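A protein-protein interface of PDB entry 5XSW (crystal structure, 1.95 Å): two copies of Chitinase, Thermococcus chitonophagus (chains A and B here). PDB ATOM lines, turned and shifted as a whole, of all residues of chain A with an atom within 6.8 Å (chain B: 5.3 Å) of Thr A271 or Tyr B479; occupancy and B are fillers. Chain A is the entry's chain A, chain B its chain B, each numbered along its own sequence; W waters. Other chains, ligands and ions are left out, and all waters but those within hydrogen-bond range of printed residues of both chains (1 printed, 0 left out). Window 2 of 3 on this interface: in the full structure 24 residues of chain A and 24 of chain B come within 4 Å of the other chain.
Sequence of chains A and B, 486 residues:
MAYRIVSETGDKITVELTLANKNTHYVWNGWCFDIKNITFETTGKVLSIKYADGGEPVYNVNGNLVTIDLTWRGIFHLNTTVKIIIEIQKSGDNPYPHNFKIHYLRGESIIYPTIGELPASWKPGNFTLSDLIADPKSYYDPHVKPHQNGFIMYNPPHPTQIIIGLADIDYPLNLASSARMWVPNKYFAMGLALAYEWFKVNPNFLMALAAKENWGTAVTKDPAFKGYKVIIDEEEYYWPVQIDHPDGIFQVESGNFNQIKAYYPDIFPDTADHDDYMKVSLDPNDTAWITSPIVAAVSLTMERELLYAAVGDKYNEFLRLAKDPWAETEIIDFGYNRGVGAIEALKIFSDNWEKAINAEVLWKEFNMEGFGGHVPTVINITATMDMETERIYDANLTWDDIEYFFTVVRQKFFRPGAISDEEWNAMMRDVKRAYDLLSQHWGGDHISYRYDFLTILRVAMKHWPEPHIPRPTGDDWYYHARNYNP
The side-chain carboxylate (OD1) of Asp A270 lies within salt-bridge range of the guanidinium group (NH2) of Arg A415, at 2.9 Å.
The side-chain amino group of Lys A261 sits at hydrogen-bond distance from the backbone carbonyl oxygen of Ala A272 (2.6 Å).
O of Tyr B479 is in hydrogen-bond range of ND2 of Asn B483 (2.6 Å).
OD2 of Asp A273 lies within hydrogen-bond range of N of Asp A276 (2.9 Å).
O of Asp A270 is in hydrogen-bond range of NZ of Lys A261, at 3.0 Å.
No position is printed for both chains.
Of chain A, only Asp A270, Thr A271 and Asp A273 come within 4 Å of Tyr B479.
Printed residues of chain B within 4 Å of Asp A273: Tyr B479, His B480 and Asn B483.
Of the printed residues of chain A, His B480 touches Asp A273 (3.7 Å).
Of the printed residues of chain A, Asp B476 touches Lys A261 (2.9 Å).
The nearest residue of chain A that does not touch Tyr B479 is Lys A261 (4.4 Å).
Of the 14 printed residues of chain A, 4 touch a printed residue of chain B.
Among the printed residues, 6 pairs touch across the chains.
Among the printed residues, Asp or Glu carboxylates within 4 Å of a Lys or Arg side-chain nitrogen of the other chain: Lys A261 with Asp B476 (2.9 Å).
Among the printed residues, merely in contact across the chains: Asp A270 with Tyr B479 (3.3 Å), Thr A271 with Tyr B479 (3.5 Å), Asp A273 with His B480 (3.7 Å) and Asp A273 with Asn B483 (3.7 Å).
Water W1 lies within hydrogen-bond range of O of Asp B476 (3.3 Å), NZ of Lys A261 (3.4 Å) and O of Ala A272 (3.5 Å).
The side-chain carboxylate of Asp A273 sits close to the backbone carbonyl oxygen of Tyr B479, 3.2 Å away.
The side-chain amino group (NZ) of Lys A261 is in salt-bridge range of the side-chain carboxylate (OD1) of Asp B476 (2.9 Å).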
ATOM      1  N   PHE A 257      24.129 -25.110 -15.569  1.00  0.00           N
ATOM      2  CA  PHE A 257      22.958 -24.638 -16.336  1.00  0.00           C
ATOM      3  C   PHE A 257      21.744 -25.485 -16.094  1.00  0.00           C
ATOM      4  O   PHE A 257      20.605 -24.986 -15.904  1.00  0.00           O
ATOM      5  CB  PHE A 257      23.297 -24.618 -17.869  1.00  0.00           C
ATOM      6  CG  PHE A 257      22.262 -23.966 -18.702  1.00  0.00           C
ATOM      7  CD1 PHE A 257      22.315 -22.594 -18.927  1.00  0.00           C
ATOM      8  CD2 PHE A 257      21.235 -24.719 -19.293  1.00  0.00           C
ATOM      9  CE1 PHE A 257      21.331 -21.923 -19.744  1.00  0.00           C
ATOM     10  CE2 PHE A 257      20.262 -24.111 -20.130  1.00  0.00           C
ATOM     11  CZ  PHE A 257      20.272 -22.706 -20.343  1.00  0.00           C
ATOM     12  N   LYS A 261      18.275 -24.074 -14.282  1.00  0.00           N
ATOM     13  CA  LYS A 261      17.004 -24.361 -14.918  1.00  0.00           C
ATOM     14  C   LYS A 261      16.034 -25.126 -13.992  1.00  0.00           C
ATOM     15  O   LYS A 261      14.824 -24.800 -13.899  1.00  0.00           O
ATOM     16  CB  LYS A 261      17.281 -25.179 -16.219  1.00  0.00           C
ATOM     17  CG  LYS A 261      16.262 -25.258 -17.210  1.00  0.00           C
ATOM     18  CD  LYS A 261      16.846 -26.005 -18.486  1.00  0.00           C
ATOM     19  CE  LYS A 261      15.667 -26.601 -19.207  1.00  0.00           C
ATOM     20  NZ  LYS A 261      16.216 -27.297 -20.410  1.00  0.00           N
ATOM     21  N   PHE A 268      13.301 -19.965 -16.561  1.00  0.00           N
ATOM     22  CA  PHE A 268      13.707 -20.754 -17.740  1.00  0.00           C
ATOM     23  C   PHE A 268      12.587 -21.619 -18.264  1.00  0.00           C
ATOM     24  O   PHE A 268      12.054 -22.417 -17.500  1.00  0.00           O
ATOM     25  CB  PHE A 268      14.886 -21.662 -17.368  1.00  0.00           C
ATOM     26  CG  PHE A 268      16.123 -20.916 -17.043  1.00  0.00           C
ATOM     27  CD1 PHE A 268      16.942 -20.412 -18.057  1.00  0.00           C
ATOM     28  CD2 PHE A 268      16.488 -20.708 -15.720  1.00  0.00           C
ATOM     29  CE1 PHE A 268      18.110 -19.712 -17.752  1.00  0.00           C
ATOM     30  CE2 PHE A 268      17.630 -20.008 -15.422  1.00  0.00           C
ATOM     31  CZ  PHE A 268      18.454 -19.516 -16.430  1.00  0.00           C
ATOM     32  N   PRO A 269      12.237 -21.471 -19.570  1.00  0.00           N
ATOM     33  CA  PRO A 269      11.307 -22.458 -20.139  1.00  0.00           C
ATOM     34  C   PRO A 269      11.980 -23.834 -20.254  1.00  0.00           C
ATOM     35  O   PRO A 269      13.212 -23.924 -20.250  1.00  0.00           O
ATOM     36  CB  PRO A 269      10.966 -21.864 -21.523  1.00  0.00           C
ATOM     37  CG  PRO A 269      12.236 -21.082 -21.934  1.00  0.00           C
ATOM     38  CD  PRO A 269      12.778 -20.535 -20.572  1.00  0.00           C
ATOM     39  N   ASP A 270      11.189 -24.895 -20.383  1.00  0.00           N
ATOM     40  CA  ASP A 270      11.740 -26.248 -20.438  1.00  0.00           C
ATOM     41  C   ASP A 270      12.631 -26.460 -21.662  1.00  0.00           C
ATOM     42  O   ASP A 270      13.449 -27.378 -21.652  1.00  0.00           O
ATOM     43  CB  ASP A 270      10.596 -27.297 -20.468  1.00  0.00           C
ATOM     44  CG  ASP A 270       9.829 -27.388 -19.115  1.00  0.00           C
ATOM     45  OD1 ASP A 270      10.385 -27.005 -18.063  1.00  0.00           O
ATOM     46  OD2 ASP A 270       8.677 -27.863 -19.107  1.00  0.00           O
ATOM     47  N   THR A 271      12.459 -25.607 -22.682  1.00  0.00           N
ATOM     48  CA  THR A 271      13.225 -25.704 -23.938  1.00  0.00           C
ATOM     49  C   THR A 271      14.639 -25.156 -23.811  1.00  0.00           C
ATOM     50  O   THR A 271      15.448 -25.325 -24.704  1.00  0.00           O
ATOM     51  CB  THR A 271      12.549 -24.932 -25.068  1.00  0.00           C
ATOM     52  OG1 THR A 271      12.205 -23.609 -24.613  1.00  0.00           O
ATOM     53  CG2 THR A 271      11.276 -25.660 -25.549  1.00  0.00           C
ATOM     54  N   ALA A 272      14.954 -24.480 -22.706  1.00  0.00           N
ATOM     55  CA  ALA A 272      16.228 -23.728 -22.633  1.00  0.00           C
ATOM     56  C   ALA A 272      17.400 -24.691 -22.752  1.00  0.00           C
ATOM     57  O   ALA A 272      17.482 -25.661 -22.017  1.00  0.00           O
ATOM     58  CB  ALA A 272      16.340 -22.946 -21.284  1.00  0.00           C
ATOM     59  N   ASP A 273      18.322 -24.382 -23.636  1.00  0.00           N
ATOM     60  CA  ASP A 273      19.440 -25.257 -23.942  1.00  0.00           C
ATOM     61  C   ASP A 273      20.766 -24.542 -23.656  1.00  0.00           C
ATOM     62  O   ASP A 273      20.937 -23.383 -24.046  1.00  0.00           O
ATOM     63  CB  ASP A 273      19.392 -25.664 -25.444  1.00  0.00           C
ATOM     64  CG  ASP A 273      20.709 -26.210 -25.908  1.00  0.00           C
ATOM     65  OD1 ASP A 273      21.058 -27.319 -25.456  1.00  0.00           O
ATOM     66  OD2 ASP A 273      21.440 -25.510 -26.620  1.00  0.00           O
ATOM     67  N   HIS A 274      21.705 -25.235 -23.021  1.00  0.00           N
ATOM     68  CA  HIS A 274      22.976 -24.629 -22.598  1.00  0.00           C
ATOM     69  C   HIS A 274      23.747 -23.898 -23.715  1.00  0.00           C
ATOM     70  O   HIS A 274      24.081 -22.673 -23.619  1.00  0.00           O
ATOM     71  CB  HIS A 274      23.870 -25.713 -21.978  1.00  0.00           C
ATOM     72  CG  HIS A 274      25.283 -25.259 -21.759  1.00  0.00           C
ATOM     73  ND1 HIS A 274      26.275 -25.408 -22.714  1.00  0.00           N
ATOM     74  CD2 HIS A 274      25.858 -24.615 -20.723  1.00  0.00           C
ATOM     75  CE1 HIS A 274      27.398 -24.871 -22.269  1.00  0.00           C
ATOM     76  NE2 HIS A 274      27.187 -24.431 -21.040  1.00  0.00           N
ATOM     77  N   ASP A 276      22.823 -22.991 -26.677  1.00  0.00           N
ATOM     78  CA  ASP A 276      22.072 -21.898 -27.260  1.00  0.00           C
ATOM     79  C   ASP A 276      22.108 -20.587 -26.398  1.00  0.00           C
ATOM     80  O   ASP A 276      22.100 -19.457 -26.948  1.00  0.00           O
ATOM     81  CB  ASP A 276      20.608 -22.295 -27.455  1.00  0.00           C
ATOM     82  CG  ASP A 276      19.765 -21.152 -28.107  1.00  0.00           C
ATOM     83  OD1 ASP A 276      20.265 -20.586 -29.088  1.00  0.00           O
ATOM     84  OD2 ASP A 276      18.618 -20.806 -27.664  1.00  0.00           O
ATOM     85  N   TYR A 277      22.110 -20.743 -25.066  1.00  0.00           N
ATOM     86  CA  TYR A 277      22.041 -19.583 -24.154  1.00  0.00           C
ATOM     87  C   TYR A 277      23.418 -19.008 -23.892  1.00  0.00           C
ATOM     88  O   TYR A 277      23.511 -17.831 -23.603  1.00  0.00           O
ATOM     89  CB  TYR A 277      21.386 -19.949 -22.801  1.00  0.00           C
ATOM     90  CG  TYR A 277      19.859 -19.954 -22.858  1.00  0.00           C
ATOM     91  CD1 TYR A 277      19.170 -20.678 -23.857  1.00  0.00           C
ATOM     92  CD2 TYR A 277      19.114 -19.213 -21.947  1.00  0.00           C
ATOM     93  CE1 TYR A 277      17.799 -20.677 -23.911  1.00  0.00           C
ATOM     94  CE2 TYR A 277      17.743 -19.222 -21.969  1.00  0.00           C
ATOM     95  CZ  TYR A 277      17.085 -19.947 -22.980  1.00  0.00           C
ATOM     96  OH  TYR A 277      15.716 -19.966 -23.038  1.00  0.00           O
ATOM     97  N   GLN A 411      11.520 -14.687 -26.084  1.00  0.00           N
ATOM     98  CA  GLN A 411      11.842 -16.037 -26.575  1.00  0.00           C
ATOM     99  C   GLN A 411      12.579 -16.894 -25.561  1.00  0.00           C
ATOM    100  O   GLN A 411      12.411 -18.123 -25.512  1.00  0.00           O
ATOM    101  CB  GLN A 411      12.728 -15.970 -27.818  1.00  0.00           C
ATOM    102  CG  GLN A 411      12.028 -15.403 -29.074  1.00  0.00           C
ATOM    103  CD  GLN A 411      13.022 -15.098 -30.234  1.00  0.00           C
ATOM    104  OE1 GLN A 411      14.236 -15.358 -30.132  1.00  0.00           O
ATOM    105  NE2 GLN A 411      12.497 -14.548 -31.328  1.00  0.00           N
ATOM    106  N   LYS A 412      13.466 -16.271 -24.795  1.00  0.00           N
ATOM    107  CA  LYS A 412      14.372 -17.073 -23.971  1.00  0.00           C
ATOM    108  C   LYS A 412      14.057 -17.148 -22.464  1.00  0.00           C
ATOM    109  O   LYS A 412      14.549 -18.054 -21.789  1.00  0.00           O
ATOM    110  CB  LYS A 412      15.800 -16.548 -24.140  1.00  0.00           C
ATOM    111  CG  LYS A 412      16.185 -16.460 -25.667  1.00  0.00           C
ATOM    112  CD  LYS A 412      16.264 -17.872 -26.288  1.00  0.00           C
ATOM    113  CE  LYS A 412      16.652 -17.776 -27.830  1.00  0.00           C
ATOM    114  NZ  LYS A 412      16.747 -19.178 -28.366  1.00  0.00           N
ATOM    115  N   ARG A 415       8.006 -18.451 -18.724  1.00  0.00           N
ATOM    116  CA  ARG A 415       7.301 -19.675 -19.085  1.00  0.00           C
ATOM    117  C   ARG A 415       5.933 -19.210 -19.584  1.00  0.00           C
ATOM    118  O   ARG A 415       5.451 -18.157 -19.168  1.00  0.00           O
ATOM    119  CB  ARG A 415       7.271 -20.576 -17.821  1.00  0.00           C
ATOM    120  CG  ARG A 415       6.625 -21.895 -17.828  1.00  0.00           C
ATOM    121  CD  ARG A 415       6.929 -22.631 -16.512  1.00  0.00           C
ATOM    122  NE  ARG A 415       8.334 -23.050 -16.484  1.00  0.00           N
ATOM    123  CZ  ARG A 415       8.761 -24.290 -16.669  1.00  0.00           C
ATOM    124  NH1 ARG A 415       7.891 -25.285 -16.861  1.00  0.00           N
ATOM    125  NH2 ARG A 415      10.071 -24.532 -16.663  1.00  0.00           N
ATOM    126  N   TRP B  72      11.024 -29.846 -32.283  1.00  0.00           N
ATOM    127  CA  TRP B  72      10.507 -29.539 -30.948  1.00  0.00           C
ATOM    128  C   TRP B  72       9.571 -30.610 -30.385  1.00  0.00           C
ATOM    129  O   TRP B  72       9.336 -30.643 -29.159  1.00  0.00           O
ATOM    130  CB  TRP B  72       9.826 -28.159 -30.977  1.00  0.00           C
ATOM    131  CG  TRP B  72       8.526 -28.123 -31.729  1.00  0.00           C
ATOM    132  CD1 TRP B  72       8.347 -27.870 -33.087  1.00  0.00           C
ATOM    133  CD2 TRP B  72       7.219 -28.368 -31.189  1.00  0.00           C
ATOM    134  NE1 TRP B  72       7.005 -27.940 -33.396  1.00  0.00           N
ATOM    135  CE2 TRP B  72       6.291 -28.232 -32.258  1.00  0.00           C
ATOM    136  CE3 TRP B  72       6.738 -28.674 -29.909  1.00  0.00           C
ATOM    137  CZ2 TRP B  72       4.917 -28.392 -32.077  1.00  0.00           C
ATOM    138  CZ3 TRP B  72       5.375 -28.826 -29.727  1.00  0.00           C
ATOM    139  CH2 TRP B  72       4.477 -28.699 -30.814  1.00  0.00           C
ATOM    140  N   ILE B  75      10.229 -35.289 -27.904  1.00  0.00           N
ATOM    141  CA  ILE B  75      10.268 -35.821 -26.522  1.00  0.00           C
ATOM    142  C   ILE B  75       8.970 -36.495 -26.134  1.00  0.00           C
ATOM    143  O   ILE B  75       7.892 -35.895 -26.241  1.00  0.00           O
ATOM    144  CB  ILE B  75      10.586 -34.674 -25.454  1.00  0.00           C
ATOM    145  CG1 ILE B  75      11.955 -34.048 -25.697  1.00  0.00           C
ATOM    146  CG2 ILE B  75      10.552 -35.246 -24.035  1.00  0.00           C
ATOM    147  CD1 ILE B  75      12.059 -32.604 -25.208  1.00  0.00           C
ATOM    148  N   ASP B 475      13.917 -34.145 -20.983  1.00  0.00           N
ATOM    149  CA  ASP B 475      13.965 -32.910 -21.731  1.00  0.00           C
ATOM    150  C   ASP B 475      15.353 -32.352 -21.868  1.00  0.00           C
ATOM    151  O   ASP B 475      15.770 -31.910 -22.971  1.00  0.00           O
ATOM    152  CB  ASP B 475      13.062 -31.831 -21.067  1.00  0.00           C
ATOM    153  CG  ASP B 475      11.550 -32.127 -21.197  1.00  0.00           C
ATOM    154  OD1 ASP B 475      11.065 -33.189 -20.801  1.00  0.00           O
ATOM    155  OD2 ASP B 475      10.826 -31.256 -21.710  1.00  0.00           O
ATOM    156  N   ASP B 476      16.054 -32.254 -20.737  1.00  0.00           N
ATOM    157  CA  ASP B 476      17.386 -31.651 -20.762  1.00  0.00           C
ATOM    158  C   ASP B 476      18.331 -32.475 -21.685  1.00  0.00           C
ATOM    159  O   ASP B 476      19.114 -31.936 -22.437  1.00  0.00           O
ATOM    160  CB  ASP B 476      18.023 -31.628 -19.346  1.00  0.00           C
ATOM    161  CG  ASP B 476      17.305 -30.614 -18.366  1.00  0.00           C
ATOM    162  OD1 ASP B 476      16.808 -29.610 -18.853  1.00  0.00           O
ATOM    163  OD2 ASP B 476      17.283 -30.859 -17.167  1.00  0.00           O
ATOM    164  N   TRP B 477      18.287 -33.788 -21.538  1.00  0.00           N
ATOM    165  CA  TRP B 477      19.103 -34.623 -22.464  1.00  0.00           C
ATOM    166  C   TRP B 477      18.808 -34.301 -23.914  1.00  0.00           C
ATOM    167  O   TRP B 477      19.705 -34.145 -24.768  1.00  0.00           O
ATOM    168  CB  TRP B 477      18.836 -36.116 -22.184  1.00  0.00           C
ATOM    169  CG  TRP B 477      19.664 -37.007 -23.090  1.00  0.00           C
ATOM    170  CD1 TRP B 477      19.208 -37.723 -24.221  1.00  0.00           C
ATOM    171  CD2 TRP B 477      21.090 -37.241 -23.009  1.00  0.00           C
ATOM    172  NE1 TRP B 477      20.277 -38.392 -24.795  1.00  0.00           N
ATOM    173  CE2 TRP B 477      21.430 -38.134 -24.079  1.00  0.00           C
ATOM    174  CE3 TRP B 477      22.100 -36.827 -22.126  1.00  0.00           C
ATOM    175  CZ2 TRP B 477      22.718 -38.574 -24.285  1.00  0.00           C
ATOM    176  CZ3 TRP B 477      23.411 -37.294 -22.332  1.00  0.00           C
ATOM    177  CH2 TRP B 477      23.692 -38.187 -23.394  1.00  0.00           C
ATOM    178  N   TYR B 478      17.525 -34.123 -24.191  1.00  0.00           N
ATOM    179  CA  TYR B 478      17.113 -33.921 -25.588  1.00  0.00           C
ATOM    180  C   TYR B 478      17.784 -32.681 -26.209  1.00  0.00           C
ATOM    181  O   TYR B 478      18.496 -32.769 -27.206  1.00  0.00           O
ATOM    182  CB  TYR B 478      15.593 -33.794 -25.649  1.00  0.00           C
ATOM    183  CG  TYR B 478      15.072 -33.753 -27.051  1.00  0.00           C
ATOM    184  CD1 TYR B 478      14.989 -34.937 -27.813  1.00  0.00           C
ATOM    185  CD2 TYR B 478      14.714 -32.543 -27.644  1.00  0.00           C
ATOM    186  CE1 TYR B 478      14.509 -34.907 -29.173  1.00  0.00           C
ATOM    187  CE2 TYR B 478      14.216 -32.498 -28.972  1.00  0.00           C
ATOM    188  CZ  TYR B 478      14.111 -33.688 -29.719  1.00  0.00           C
ATOM    189  OH  TYR B 478      13.654 -33.643 -31.017  1.00  0.00           O
ATOM    190  N   TYR B 479      17.612 -31.518 -25.573  1.00  0.00           N
ATOM    191  CA  TYR B 479      18.201 -30.292 -26.089  1.00  0.00           C
ATOM    192  C   TYR B 479      19.691 -30.352 -26.082  1.00  0.00           C
ATOM    193  O   TYR B 479      20.349 -29.975 -27.059  1.00  0.00           O
ATOM    194  CB  TYR B 479      17.695 -29.089 -25.286  1.00  0.00           C
ATOM    195  CG  TYR B 479      16.196 -29.027 -25.394  1.00  0.00           C
ATOM    196  CD1 TYR B 479      15.582 -28.902 -26.645  1.00  0.00           C
ATOM    197  CD2 TYR B 479      15.415 -29.178 -24.291  1.00  0.00           C
ATOM    198  CE1 TYR B 479      14.204 -28.902 -26.750  1.00  0.00           C
ATOM    199  CE2 TYR B 479      14.069 -29.185 -24.366  1.00  0.00           C
ATOM    200  CZ  TYR B 479      13.465 -29.037 -25.612  1.00  0.00           C
ATOM    201  OH  TYR B 479      12.109 -29.058 -25.644  1.00  0.00           O
ATOM    202  N   HIS B 480      20.248 -30.933 -25.034  1.00  0.00           N
ATOM    203  CA  HIS B 480      21.698 -30.919 -24.942  1.00  0.00           C
ATOM    204  C   HIS B 480      22.359 -31.801 -26.018  1.00  0.00           C
ATOM    205  O   HIS B 480      23.288 -31.354 -26.725  1.00  0.00           O
ATOM    206  CB  HIS B 480      22.138 -31.398 -23.548  1.00  0.00           C
ATOM    207  CG  HIS B 480      23.578 -31.166 -23.275  1.00  0.00           C
ATOM    208  ND1 HIS B 480      24.309 -31.961 -22.427  1.00  0.00           N
ATOM    209  CD2 HIS B 480      24.429 -30.227 -23.742  1.00  0.00           C
ATOM    210  CE1 HIS B 480      25.552 -31.517 -22.377  1.00  0.00           C
ATOM    211  NE2 HIS B 480      25.658 -30.483 -23.190  1.00  0.00           N
ATOM    212  N   ALA B 481      21.902 -33.059 -26.113  1.00  0.00           N
ATOM    213  CA  ALA B 481      22.541 -34.007 -27.033  1.00  0.00           C
ATOM    214  C   ALA B 481      22.220 -33.646 -28.482  1.00  0.00           C
ATOM    215  O   ALA B 481      23.051 -33.852 -29.359  1.00  0.00           O
ATOM    216  CB  ALA B 481      22.123 -35.485 -26.718  1.00  0.00           C
ATOM    217  N   ARG B 482      21.064 -33.049 -28.739  1.00  0.00           N
ATOM    218  CA  ARG B 482      20.778 -32.665 -30.138  1.00  0.00           C
ATOM    219  C   ARG B 482      21.686 -31.533 -30.571  1.00  0.00           C
ATOM    220  O   ARG B 482      22.016 -31.422 -31.742  1.00  0.00           O
ATOM    221  CB  ARG B 482      19.322 -32.242 -30.330  1.00  0.00           C
ATOM    222  CG  ARG B 482      18.386 -33.433 -30.344  1.00  0.00           C
ATOM    223  CD  ARG B 482      16.994 -32.974 -30.743  1.00  0.00           C
ATOM    224  NE  ARG B 482      16.963 -32.160 -31.952  1.00  0.00           N
ATOM    225  CZ  ARG B 482      16.440 -32.553 -33.121  1.00  0.00           C
ATOM    226  NH1 ARG B 482      15.885 -33.749 -33.240  1.00  0.00           N
ATOM    227  NH2 ARG B 482      16.468 -31.733 -34.170  1.00  0.00           N
ATOM    228  N   ASN B 483      22.110 -30.692 -29.628  1.00  0.00           N
ATOM    229  CA  ASN B 483      22.917 -29.521 -29.999  1.00  0.00           C
ATOM    230  C   ASN B 483      24.432 -29.688 -29.804  1.00  0.00           C
ATOM    231  O   ASN B 483      25.192 -28.740 -29.978  1.00  0.00           O
ATOM    232  CB  ASN B 483      22.373 -28.285 -29.245  1.00  0.00           C
ATOM    233  CG  ASN B 483      20.955 -27.921 -29.746  1.00  0.00           C
ATOM    234  OD1 ASN B 483      20.799 -27.450 -30.869  1.00  0.00           O
ATOM    235  ND2 ASN B 483      19.921 -28.241 -28.960  1.00  0.00           N
ATOM    236  N   TYR B 484      24.875 -30.911 -29.506  1.00  0.00           N
ATOM    237  CA  TYR B 484      26.248 -31.155 -29.083  1.00  0.00           C
ATOM    238  C   TYR B 484      27.077 -31.471 -30.321  1.00  0.00           C
ATOM    239  O   TYR B 484      26.766 -32.429 -31.032  1.00  0.00           O
ATOM    240  CB  TYR B 484      26.277 -32.320 -28.053  1.00  0.00           C
ATOM    241  CG  TYR B 484      27.602 -32.455 -27.358  1.00  0.00           C
ATOM    242  CD1 TYR B 484      28.041 -31.469 -26.455  1.00  0.00           C
ATOM    243  CD2 TYR B 484      28.400 -33.567 -27.573  1.00  0.00           C
ATOM    244  CE1 TYR B 484      29.265 -31.607 -25.824  1.00  0.00           C
ATOM    245  CE2 TYR B 484      29.602 -33.735 -26.946  1.00  0.00           C
ATOM    246  CZ  TYR B 484      30.036 -32.759 -26.050  1.00  0.00           C
ATOM    247  OH  TYR B 484      31.259 -32.936 -25.441  1.00  0.00           O
HETATM  248  O   HOH W   1      19.000 -28.764 -21.647  1.00  0.00           O
